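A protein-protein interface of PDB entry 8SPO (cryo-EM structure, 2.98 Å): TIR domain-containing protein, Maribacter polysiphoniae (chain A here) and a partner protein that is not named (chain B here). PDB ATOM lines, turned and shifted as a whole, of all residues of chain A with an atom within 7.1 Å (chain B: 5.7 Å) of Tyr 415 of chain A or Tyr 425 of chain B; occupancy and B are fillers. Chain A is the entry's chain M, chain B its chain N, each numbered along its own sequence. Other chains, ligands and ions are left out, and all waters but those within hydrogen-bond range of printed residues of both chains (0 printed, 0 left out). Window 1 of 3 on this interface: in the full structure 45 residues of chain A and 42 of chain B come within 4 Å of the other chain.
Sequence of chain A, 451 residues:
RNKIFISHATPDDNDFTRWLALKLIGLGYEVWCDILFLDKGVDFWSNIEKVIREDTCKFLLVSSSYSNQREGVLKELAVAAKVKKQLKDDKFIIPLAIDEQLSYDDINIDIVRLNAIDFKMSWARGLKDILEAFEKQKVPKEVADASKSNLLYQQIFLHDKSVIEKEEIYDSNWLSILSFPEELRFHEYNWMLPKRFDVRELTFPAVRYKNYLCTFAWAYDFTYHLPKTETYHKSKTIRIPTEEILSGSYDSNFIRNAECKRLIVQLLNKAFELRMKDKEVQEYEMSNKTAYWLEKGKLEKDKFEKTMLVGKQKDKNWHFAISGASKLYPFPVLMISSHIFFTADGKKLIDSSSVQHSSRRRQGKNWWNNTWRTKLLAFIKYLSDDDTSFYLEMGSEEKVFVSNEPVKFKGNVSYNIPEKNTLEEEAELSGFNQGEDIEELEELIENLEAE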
ATOM      1  N   SER A 162      14.390  16.830  -4.223  1.00  0.00           N
ATOM      2  CA  SER A 162      13.042  17.323  -4.627  1.00  0.00           C
ATOM      3  C   SER A 162      12.436  18.237  -3.556  1.00  0.00           C
ATOM      4  O   SER A 162      13.028  18.341  -2.462  1.00  0.00           O
ATOM      5  CB  SER A 162      12.121  16.174  -4.938  1.00  0.00           C
ATOM      6  OG  SER A 162      11.982  15.321  -3.810  1.00  0.00           O
ATOM      7  N   VAL A 163      11.298  18.872  -3.866  1.00  0.00           N
ATOM      8  CA  VAL A 163      10.620  19.780  -2.894  1.00  0.00           C
ATOM      9  C   VAL A 163       9.925  18.913  -1.848  1.00  0.00           C
ATOM     10  O   VAL A 163       9.070  18.097  -2.238  1.00  0.00           O
ATOM     11  CB  VAL A 163       9.618  20.717  -3.590  1.00  0.00           C
ATOM     12  CG1 VAL A 163       8.771  21.490  -2.593  1.00  0.00           C
ATOM     13  CG2 VAL A 163      10.310  21.666  -4.555  1.00  0.00           C
ATOM     14  N   ILE A 164      10.274  19.085  -0.568  1.00  0.00           N
ATOM     15  CA  ILE A 164       9.674  18.187   0.410  1.00  0.00           C
ATOM     16  C   ILE A 164       8.646  18.967   1.214  1.00  0.00           C
ATOM     17  O   ILE A 164       8.918  20.093   1.648  1.00  0.00           O
ATOM     18  CB  ILE A 164      10.732  17.576   1.349  1.00  0.00           C
ATOM     19  CG1 ILE A 164      11.875  16.943   0.547  1.00  0.00           C
ATOM     20  CG2 ILE A 164      10.094  16.555   2.275  1.00  0.00           C
ATOM     21  CD1 ILE A 164      11.467  15.744  -0.282  1.00  0.00           C
ATOM     22  N   GLU A 165       7.471  18.374   1.408  1.00  0.00           N
ATOM     23  CA  GLU A 165       6.450  18.952   2.275  1.00  0.00           C
ATOM     24  C   GLU A 165       6.802  18.610   3.718  1.00  0.00           C
ATOM     25  O   GLU A 165       6.640  17.463   4.149  1.00  0.00           O
ATOM     26  CB  GLU A 165       5.065  18.428   1.908  1.00  0.00           C
ATOM     27  CG  GLU A 165       4.753  18.454   0.417  1.00  0.00           C
ATOM     28  CD  GLU A 165       4.463  19.850  -0.100  1.00  0.00           C
ATOM     29  OE1 GLU A 165       4.148  20.739   0.717  1.00  0.00           O
ATOM     30  OE2 GLU A 165       4.553  20.058  -1.329  1.00  0.00           O
ATOM     31  N   LYS A 166       7.281  19.600   4.466  1.00  0.00           N
ATOM     32  CA  LYS A 166       7.786  19.364   5.814  1.00  0.00           C
ATOM     33  C   LYS A 166       7.766  20.683   6.569  1.00  0.00           C
ATOM     34  O   LYS A 166       8.473  21.621   6.192  1.00  0.00           O
ATOM     35  CB  LYS A 166       9.200  18.781   5.761  1.00  0.00           C
ATOM     36  CG  LYS A 166       9.951  18.793   7.079  1.00  0.00           C
ATOM     37  CD  LYS A 166      11.310  18.127   6.940  1.00  0.00           C
ATOM     38  CE  LYS A 166      12.215  18.891   5.983  1.00  0.00           C
ATOM     39  NZ  LYS A 166      13.642  18.488   6.115  1.00  0.00           N
ATOM     40  N   GLU A 168       8.461  23.688   8.943  1.00  0.00           N
ATOM     41  CA  GLU A 168       9.619  24.251   9.617  1.00  0.00           C
ATOM     42  C   GLU A 168       9.253  25.600  10.215  1.00  0.00           C
ATOM     43  O   GLU A 168       8.260  26.224   9.835  1.00  0.00           O
ATOM     44  CB  GLU A 168      10.815  24.417   8.676  1.00  0.00           C
ATOM     45  CG  GLU A 168      11.507  23.118   8.337  1.00  0.00           C
ATOM     46  CD  GLU A 168      12.789  23.338   7.573  1.00  0.00           C
ATOM     47  OE1 GLU A 168      13.070  24.501   7.213  1.00  0.00           O
ATOM     48  OE2 GLU A 168      13.515  22.352   7.327  1.00  0.00           O
ATOM     49  N   TYR A 170      11.137  29.364  11.501  1.00  0.00           N
ATOM     50  CA  TYR A 170      12.317  30.202  11.356  1.00  0.00           C
ATOM     51  C   TYR A 170      12.343  31.282  12.430  1.00  0.00           C
ATOM     52  O   TYR A 170      11.299  31.788  12.852  1.00  0.00           O
ATOM     53  CB  TYR A 170      12.357  30.864   9.976  1.00  0.00           C
ATOM     54  CG  TYR A 170      12.092  29.930   8.819  1.00  0.00           C
ATOM     55  CD1 TYR A 170      10.800  29.667   8.394  1.00  0.00           C
ATOM     56  CD2 TYR A 170      13.137  29.321   8.142  1.00  0.00           C
ATOM     57  CE1 TYR A 170      10.554  28.820   7.333  1.00  0.00           C
ATOM     58  CE2 TYR A 170      12.902  28.475   7.080  1.00  0.00           C
ATOM     59  CZ  TYR A 170      11.610  28.227   6.680  1.00  0.00           C
ATOM     60  OH  TYR A 170      11.368  27.383   5.622  1.00  0.00           O
ATOM     61  N   ASN A 369      24.302  30.132   8.708  1.00  0.00           N
ATOM     62  CA  ASN A 369      22.998  30.462   9.276  1.00  0.00           C
ATOM     63  C   ASN A 369      22.989  30.298  10.791  1.00  0.00           C
ATOM     64  O   ASN A 369      22.581  31.209  11.524  1.00  0.00           O
ATOM     65  CB  ASN A 369      21.932  29.569   8.635  1.00  0.00           C
ATOM     66  CG  ASN A 369      20.654  29.511   9.442  1.00  0.00           C
ATOM     67  OD1 ASN A 369      20.239  30.501  10.045  1.00  0.00           O
ATOM     68  ND2 ASN A 369      20.026  28.345   9.466  1.00  0.00           N
ATOM     69  N   VAL A 413       6.968  24.243   3.347  1.00  0.00           N
ATOM     70  CA  VAL A 413       7.790  23.609   2.324  1.00  0.00           C
ATOM     71  C   VAL A 413       9.252  23.772   2.709  1.00  0.00           C
ATOM     72  O   VAL A 413       9.690  24.877   3.048  1.00  0.00           O
ATOM     73  CB  VAL A 413       7.517  24.211   0.936  1.00  0.00           C
ATOM     74  CG1 VAL A 413       8.519  23.704  -0.061  1.00  0.00           C
ATOM     75  CG2 VAL A 413       6.108  23.869   0.479  1.00  0.00           C
ATOM     76  N   SER A 414      10.002  22.674   2.660  1.00  0.00           N
ATOM     77  CA  SER A 414      11.425  22.699   2.966  1.00  0.00           C
ATOM     78  C   SER A 414      12.125  21.660   2.098  1.00  0.00           C
ATOM     79  O   SER A 414      11.515  21.034   1.227  1.00  0.00           O
ATOM     80  CB  SER A 414      11.671  22.450   4.457  1.00  0.00           C
ATOM     81  OG  SER A 414      13.022  22.716   4.788  1.00  0.00           O
ATOM     82  N   TYR A 415      13.417  21.483   2.341  1.00  0.00           N
ATOM     83  CA  TYR A 415      14.238  20.520   1.626  1.00  0.00           C
ATOM     84  C   TYR A 415      14.767  19.478   2.601  1.00  0.00           C
ATOM     85  O   TYR A 415      14.642  19.609   3.822  1.00  0.00           O
ATOM     86  CB  TYR A 415      15.395  21.209   0.884  1.00  0.00           C
ATOM     87  CG  TYR A 415      16.246  22.118   1.742  1.00  0.00           C
ATOM     88  CD1 TYR A 415      15.773  23.355   2.151  1.00  0.00           C
ATOM     89  CD2 TYR A 415      17.519  21.740   2.142  1.00  0.00           C
ATOM     90  CE1 TYR A 415      16.537  24.189   2.930  1.00  0.00           C
ATOM     91  CE2 TYR A 415      18.295  22.571   2.923  1.00  0.00           C
ATOM     92  CZ  TYR A 415      17.797  23.794   3.314  1.00  0.00           C
ATOM     93  OH  TYR A 415      18.554  24.633   4.092  1.00  0.00           O
ATOM     94  N   ASN A 416      15.368  18.432   2.043  1.00  0.00           N
ATOM     95  CA  ASN A 416      15.750  17.251   2.798  1.00  0.00           C
ATOM     96  C   ASN A 416      17.174  17.321   3.332  1.00  0.00           C
ATOM     97  O   ASN A 416      17.666  16.323   3.870  1.00  0.00           O
ATOM     98  CB  ASN A 416      15.583  16.004   1.923  1.00  0.00           C
ATOM     99  CG  ASN A 416      15.068  14.807   2.697  1.00  0.00           C
ATOM    100  OD1 ASN A 416      14.829  14.883   3.902  1.00  0.00           O
ATOM    101  ND2 ASN A 416      14.891  13.692   2.000  1.00  0.00           N
ATOM    102  N   ILE A 417      17.837  18.466   3.198  1.00  0.00           N
ATOM    103  CA  ILE A 417      19.208  18.674   3.666  1.00  0.00           C
ATOM    104  C   ILE A 417      20.063  17.449   3.356  1.00  0.00           C
ATOM    105  O   ILE A 417      20.777  16.953   4.238  1.00  0.00           O
ATOM    106  CB  ILE A 417      19.227  19.027   5.167  1.00  0.00           C
ATOM    107  CG1 ILE A 417      20.628  19.478   5.598  1.00  0.00           C
ATOM    108  CG2 ILE A 417      18.719  17.867   6.039  1.00  0.00           C
ATOM    109  CD1 ILE A 417      20.637  20.273   6.881  1.00  0.00           C
ATOM    110  N   PRO A 418      20.049  16.940   2.121  1.00  0.00           N
ATOM    111  CA  PRO A 418      20.806  15.708   1.832  1.00  0.00           C
ATOM    112  C   PRO A 418      22.278  15.986   1.551  1.00  0.00           C
ATOM    113  O   PRO A 418      22.755  15.919   0.415  1.00  0.00           O
ATOM    114  CB  PRO A 418      20.065  15.150   0.613  1.00  0.00           C
ATOM    115  CG  PRO A 418      19.572  16.374  -0.115  1.00  0.00           C
ATOM    116  CD  PRO A 418      19.469  17.509   0.889  1.00  0.00           C
ATOM    117  N   GLU A 419      23.008  16.308   2.617  1.00  0.00           N
ATOM    118  CA  GLU A 419      24.437  16.626   2.550  1.00  0.00           C
ATOM    119  C   GLU A 419      24.790  17.407   1.288  1.00  0.00           C
ATOM    120  O   GLU A 419      23.981  18.186   0.781  1.00  0.00           O
ATOM    121  CB  GLU A 419      25.274  15.343   2.626  1.00  0.00           C
ATOM    122  CG  GLU A 419      25.411  14.579   1.312  1.00  0.00           C
ATOM    123  CD  GLU A 419      25.699  13.103   1.513  1.00  0.00           C
ATOM    124  OE1 GLU A 419      25.640  12.631   2.668  1.00  0.00           O
ATOM    125  OE2 GLU A 419      25.984  12.413   0.513  1.00  0.00           O
ATOM    126  N   LYS B 398      17.025  29.540   9.677  1.00  0.00           N
ATOM    127  CA  LYS B 398      16.644  28.168   9.986  1.00  0.00           C
ATOM    128  C   LYS B 398      17.212  27.781  11.344  1.00  0.00           C
ATOM    129  O   LYS B 398      18.399  27.987  11.613  1.00  0.00           O
ATOM    130  CB  LYS B 398      17.147  27.213   8.906  1.00  0.00           C
ATOM    131  CG  LYS B 398      16.079  26.761   7.925  1.00  0.00           C
ATOM    132  CD  LYS B 398      16.597  25.695   6.966  1.00  0.00           C
ATOM    133  CE  LYS B 398      16.911  24.383   7.675  1.00  0.00           C
ATOM    134  NZ  LYS B 398      17.540  23.388   6.766  1.00  0.00           N
ATOM    135  N   TYR B 403      22.134  25.578   6.595  1.00  0.00           N
ATOM    136  CA  TYR B 403      21.756  26.020   5.262  1.00  0.00           C
ATOM    137  C   TYR B 403      20.612  27.022   5.365  1.00  0.00           C
ATOM    138  O   TYR B 403      19.826  26.996   6.316  1.00  0.00           O
ATOM    139  CB  TYR B 403      21.346  24.840   4.381  1.00  0.00           C
ATOM    140  CG  TYR B 403      22.492  23.951   3.957  1.00  0.00           C
ATOM    141  CD1 TYR B 403      23.226  24.230   2.814  1.00  0.00           C
ATOM    142  CD2 TYR B 403      22.837  22.829   4.698  1.00  0.00           C
ATOM    143  CE1 TYR B 403      24.271  23.418   2.421  1.00  0.00           C
ATOM    144  CE2 TYR B 403      23.883  22.013   4.315  1.00  0.00           C
ATOM    145  CZ  TYR B 403      24.596  22.311   3.177  1.00  0.00           C
ATOM    146  OH  TYR B 403      25.637  21.497   2.795  1.00  0.00           O
ATOM    147  N   THR B 404      20.524  27.902   4.375  1.00  0.00           N
ATOM    148  CA  THR B 404      19.649  29.061   4.443  1.00  0.00           C
ATOM    149  C   THR B 404      18.223  28.704   4.021  1.00  0.00           C
ATOM    150  O   THR B 404      17.902  27.553   3.713  1.00  0.00           O
ATOM    151  CB  THR B 404      20.205  30.193   3.579  1.00  0.00           C
ATOM    152  OG1 THR B 404      19.372  31.349   3.715  1.00  0.00           O
ATOM    153  CG2 THR B 404      20.260  29.785   2.113  1.00  0.00           C
ATOM    154  N   ILE B 405      17.351  29.715   4.006  1.00  0.00           N
ATOM    155  CA  ILE B 405      15.953  29.517   3.646  1.00  0.00           C
ATOM    156  C   ILE B 405      15.837  29.113   2.176  1.00  0.00           C
ATOM    157  O   ILE B 405      16.742  29.329   1.361  1.00  0.00           O
ATOM    158  CB  ILE B 405      15.151  30.794   3.947  1.00  0.00           C
ATOM    159  CG1 ILE B 405      13.652  30.563   3.742  1.00  0.00           C
ATOM    160  CG2 ILE B 405      15.634  31.943   3.073  1.00  0.00           C
ATOM    161  CD1 ILE B 405      12.788  31.708   4.197  1.00  0.00           C
ATOM    162  N   LEU B 406      14.697  28.517   1.839  1.00  0.00           N
ATOM    163  CA  LEU B 406      14.433  28.049   0.488  1.00  0.00           C
ATOM    164  C   LEU B 406      14.148  29.238  -0.436  1.00  0.00           C
ATOM    165  O   LEU B 406      13.933  30.368   0.008  1.00  0.00           O
ATOM    166  CB  LEU B 406      13.264  27.064   0.507  1.00  0.00           C
ATOM    167  CG  LEU B 406      12.846  26.351  -0.776  1.00  0.00           C
ATOM    168  CD1 LEU B 406      13.971  25.465  -1.276  1.00  0.00           C
ATOM    169  CD2 LEU B 406      11.594  25.538  -0.529  1.00  0.00           C
ATOM    170  N   ARG B 407      14.148  28.973  -1.746  1.00  0.00           N
ATOM    171  CA  ARG B 407      14.110  30.067  -2.713  1.00  0.00           C
ATOM    172  C   ARG B 407      12.699  30.594  -2.943  1.00  0.00           C
ATOM    173  O   ARG B 407      12.503  31.807  -3.035  1.00  0.00           O
ATOM    174  CB  ARG B 407      14.717  29.630  -4.047  1.00  0.00           C
ATOM    175  CG  ARG B 407      14.704  30.733  -5.103  1.00  0.00           C
ATOM    176  CD  ARG B 407      15.415  30.351  -6.392  1.00  0.00           C
ATOM    177  NE  ARG B 407      15.360  31.438  -7.365  1.00  0.00           N
ATOM    178  CZ  ARG B 407      14.590  31.460  -8.447  1.00  0.00           C
ATOM    179  NH1 ARG B 407      13.792  30.452  -8.755  1.00  0.00           N
ATOM    180  NH2 ARG B 407      14.615  32.529  -9.238  1.00  0.00           N
ATOM    181  N   VAL B 423      16.786  34.958  -3.505  1.00  0.00           N
ATOM    182  CA  VAL B 423      18.095  34.375  -3.255  1.00  0.00           C
ATOM    183  C   VAL B 423      17.973  33.472  -2.038  1.00  0.00           C
ATOM    184  O   VAL B 423      17.479  33.902  -0.989  1.00  0.00           O
ATOM    185  CB  VAL B 423      19.162  35.463  -3.031  1.00  0.00           C
ATOM    186  CG1 VAL B 423      20.510  34.842  -2.738  1.00  0.00           C
ATOM    187  CG2 VAL B 423      19.246  36.368  -4.245  1.00  0.00           C
ATOM    188  N   GLY B 424      18.410  32.230  -2.179  1.00  0.00           N
ATOM    189  CA  GLY B 424      18.315  31.293  -1.082  1.00  0.00           C
ATOM    190  C   GLY B 424      18.791  29.926  -1.501  1.00  0.00           C
ATOM    191  O   GLY B 424      19.466  29.774  -2.521  1.00  0.00           O
ATOM    192  N   TYR B 425      18.439  28.928  -0.698  1.00  0.00           N
ATOM    193  CA  TYR B 425      18.841  27.562  -0.994  1.00  0.00           C
ATOM    194  C   TYR B 425      18.008  27.009  -2.142  1.00  0.00           C
ATOM    195  O   TYR B 425      16.776  27.069  -2.115  1.00  0.00           O
ATOM    196  CB  TYR B 425      18.690  26.686   0.250  1.00  0.00           C
ATOM    197  CG  TYR B 425      19.219  25.283   0.073  1.00  0.00           C
ATOM    198  CD1 TYR B 425      18.422  24.279  -0.455  1.00  0.00           C
ATOM    199  CD2 TYR B 425      20.515  24.962   0.436  1.00  0.00           C
ATOM    200  CE1 TYR B 425      18.902  22.999  -0.616  1.00  0.00           C
ATOM    201  CE2 TYR B 425      21.004  23.688   0.277  1.00  0.00           C
ATOM    202  CZ  TYR B 425      20.194  22.709  -0.251  1.00  0.00           C
ATOM    203  OH  TYR B 425      20.678  21.433  -0.410  1.00  0.00           O
ATOM    204  N   VAL B 426      18.684  26.485  -3.154  1.00  0.00           N
ATOM    205  CA  VAL B 426      18.054  25.839  -4.300  1.00  0.00           C
ATOM    206  C   VAL B 426      18.323  24.342  -4.187  1.00  0.00           C
ATOM    207  O   VAL B 426      19.489  23.929  -4.237  1.00  0.00           O
ATOM    208  CB  VAL B 426      18.587  26.395  -5.631  1.00  0.00           C
ATOM    209  CG1 VAL B 426      18.083  25.559  -6.796  1.00  0.00           C
ATOM    210  CG2 VAL B 426      18.174  27.845  -5.797  1.00  0.00           C
ATOM    211  N   PRO B 427      17.300  23.500  -4.029  1.00  0.00           N
ATOM    212  CA  PRO B 427      17.568  22.075  -3.795  1.00  0.00           C
ATOM    213  C   PRO B 427      18.043  21.336  -5.028  1.00  0.00           C
ATOM    214  O   PRO B 427      18.650  20.268  -4.886  1.00  0.00           O
ATOM    215  CB  PRO B 427      16.219  21.539  -3.301  1.00  0.00           C
ATOM    216  CG  PRO B 427      15.204  22.473  -3.842  1.00  0.00           C
ATOM    217  CD  PRO B 427      15.856  23.797  -4.077  1.00  0.00           C
ATOM    218  N   GLN B 430      21.739  21.826  -4.802  1.00  0.00           N
ATOM    219  CA  GLN B 430      22.249  21.436  -3.487  1.00  0.00           C
ATOM    220  C   GLN B 430      23.150  22.516  -2.891  1.00  0.00           C
ATOM    221  O   GLN B 430      24.198  22.224  -2.314  1.00  0.00           O
ATOM    222  CB  GLN B 430      22.983  20.094  -3.551  1.00  0.00           C
ATOM    223  CG  GLN B 430      22.171  18.967  -4.170  1.00  0.00           C
ATOM    224  CD  GLN B 430      20.992  18.557  -3.317  1.00  0.00           C
ATOM    225  OE1 GLN B 430      19.906  18.282  -3.829  1.00  0.00           O
ATOM    226  NE2 GLN B 430      21.194  18.516  -2.007  1.00  0.00           N
ATOM    227  N   THR B 431      22.742  23.773  -3.024  1.00  0.00           N
ATOM    228  CA  THR B 431      23.484  24.884  -2.442  1.00  0.00           C
ATOM    229  C   THR B 431      22.626  26.140  -2.535  1.00  0.00           C
ATOM    230  O   THR B 431      21.551  26.139  -3.140  1.00  0.00           O
ATOM    231  CB  THR B 431      24.837  25.072  -3.138  1.00  0.00           C
ATOM    232  OG1 THR B 431      25.530  26.179  -2.552  1.00  0.00           O
ATOM    233  CG2 THR B 431      24.656  25.323  -4.630  1.00  0.00           C
ATOM    234  N   ALA B 432      23.119  27.215  -1.931  1.00  0.00           N
ATOM    235  CA  ALA B 432      22.445  28.504  -1.933  1.00  0.00           C
ATOM    236  C   ALA B 432      23.165  29.467  -2.866  1.00  0.00           C
ATOM    237  O   ALA B 432      24.383  29.387  -3.050  1.00  0.00           O
ATOM    238  CB  ALA B 432      22.386  29.096  -0.522  1.00  0.00           C
ATOM    239  N   LEU B 433      22.395  30.387  -3.453  1.00  0.00           N
ATOM    240  CA  LEU B 433      22.959  31.324  -4.418  1.00  0.00           C
ATOM    241  C   LEU B 433      23.799  32.411  -3.755  1.00  0.00           C
ATOM    242  O   LEU B 433      24.543  33.109  -4.450  1.00  0.00           O
ATOM    243  CB  LEU B 433      21.836  31.959  -5.238  1.00  0.00           C
ATOM    244  CG  LEU B 433      21.032  30.982  -6.102  1.00  0.00           C
ATOM    245  CD1 LEU B 433      19.833  31.677  -6.727  1.00  0.00           C
ATOM    246  CD2 LEU B 433      21.907  30.350  -7.175  1.00  0.00           C
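The backbone carbonyl oxygen of Tyr 425 of chain B lies within hydrogen-bond range of the backbone NH of Arg 407 of chain B. The side-chain carboxylate (OE2) of Glu 168 of chain A lies within hydrogen-bond range of the side-chain hydroxyl (OG) of Ser 414 of chain A (2.6 Å). OE1 of Gln 430 of chain B sits close to O of Pro 427 of chain B, at 2.6 Å. The backbone carbonyl oxygen of Ile 405 of chain B lies within hydrogen-bond range of the backbone NH of Tyr 425 of chain B (2.7 Å). NZ of Lys 166 of chain A sits at hydrogen-bond distance from O of Tyr 415 of chain A. OH of Tyr 425 of chain B lies within hydrogen-bond range of NE2 of Gln 430 of chain B (3.4 Å).
Tyr 415 of chain A touches just these residues of chain B: Lys 398 (3.1 Å), Tyr 403 (2.8 Å), Thr 404 (3.0 Å) and Tyr 425 (3.3 Å). Tyr 425 of chain B touches just one residue of chain A: Tyr 415. Printed residues of chain B within 4 Å of Tyr 170 of chain A: Lys 398 (3.7 Å). Printed residues of chain A within 4 Å of Thr 404 of chain B: Tyr 415 (3.0 Å). Printed residues of chain A within 4 Å of Lys 398 of chain B: Glu 168 (3.7 Å), Tyr 170 (3.7 Å), Asn 369 (2.7 Å) and Tyr 415 (3.1 Å). Printed residues of chain B within 4 Å of Val 413 of chain A: Leu 406. Of the printed residues of chain A, Leu 406 of chain B touches Val 413 (3.6 Å). The nearest residue of chain A that does not touch Tyr 425 of chain B is Pro 418 of chain A (4.3 Å).
O of Tyr 403 of chain B lies within hydrogen-bond range of ND2 of Asn 369 of chain A, 3.4 Å away. The backbone carbonyl oxygen (O) of Tyr 403 of chain B lies close to the side-chain hydroxyl (OH) of Tyr 415 of chain A. The backbone carbonyl oxygen (O) of Thr 404 of chain B sits at hydrogen-bond distance from the side-chain hydroxyl (OH) of Tyr 415 of chain A, at 3.0 Å. The side-chain hydroxyl (OH) of Tyr 415 of chain A is in hydrogen-bond range of the side-chain amino group (NZ) of Lys 398 of chain B (3.1 Å). The side-chain amide nitrogen (ND2) of Asn 369 of chain A sits at hydrogen-bond distance from the backbone carbonyl oxygen (O) of Lys 398 of chain B (2.7 Å).
Among the printed residues, merely in contact across the chains: Pro 418 of chain A with Gln 430 of chain B (3.3 Å), Tyr 415 of chain A with Tyr 425 of chain B (3.3 Å), Val 413 of chain A with Leu 406 of chain B (3.6 Å), Tyr 170 of chain A with Lys 398 of chain B (3.7 Å), Glu 168 of chain A with Lys 398 of chain B (3.7 Å) and Glu 419 of chain A with Gln 430 of chain B (3.96 Å).
Of the 15 printed residues of chain B, 6 touch a printed residue of chain A. Hydrophobic or aromatic side chains of chain B that line the printed part of chain A: Tyr 403, Leu 406 and Tyr 425. Among the printed residues, no Asp or Glu carboxylate lies within 4 Å of a Lys or Arg side-chain nitrogen of the other chain.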
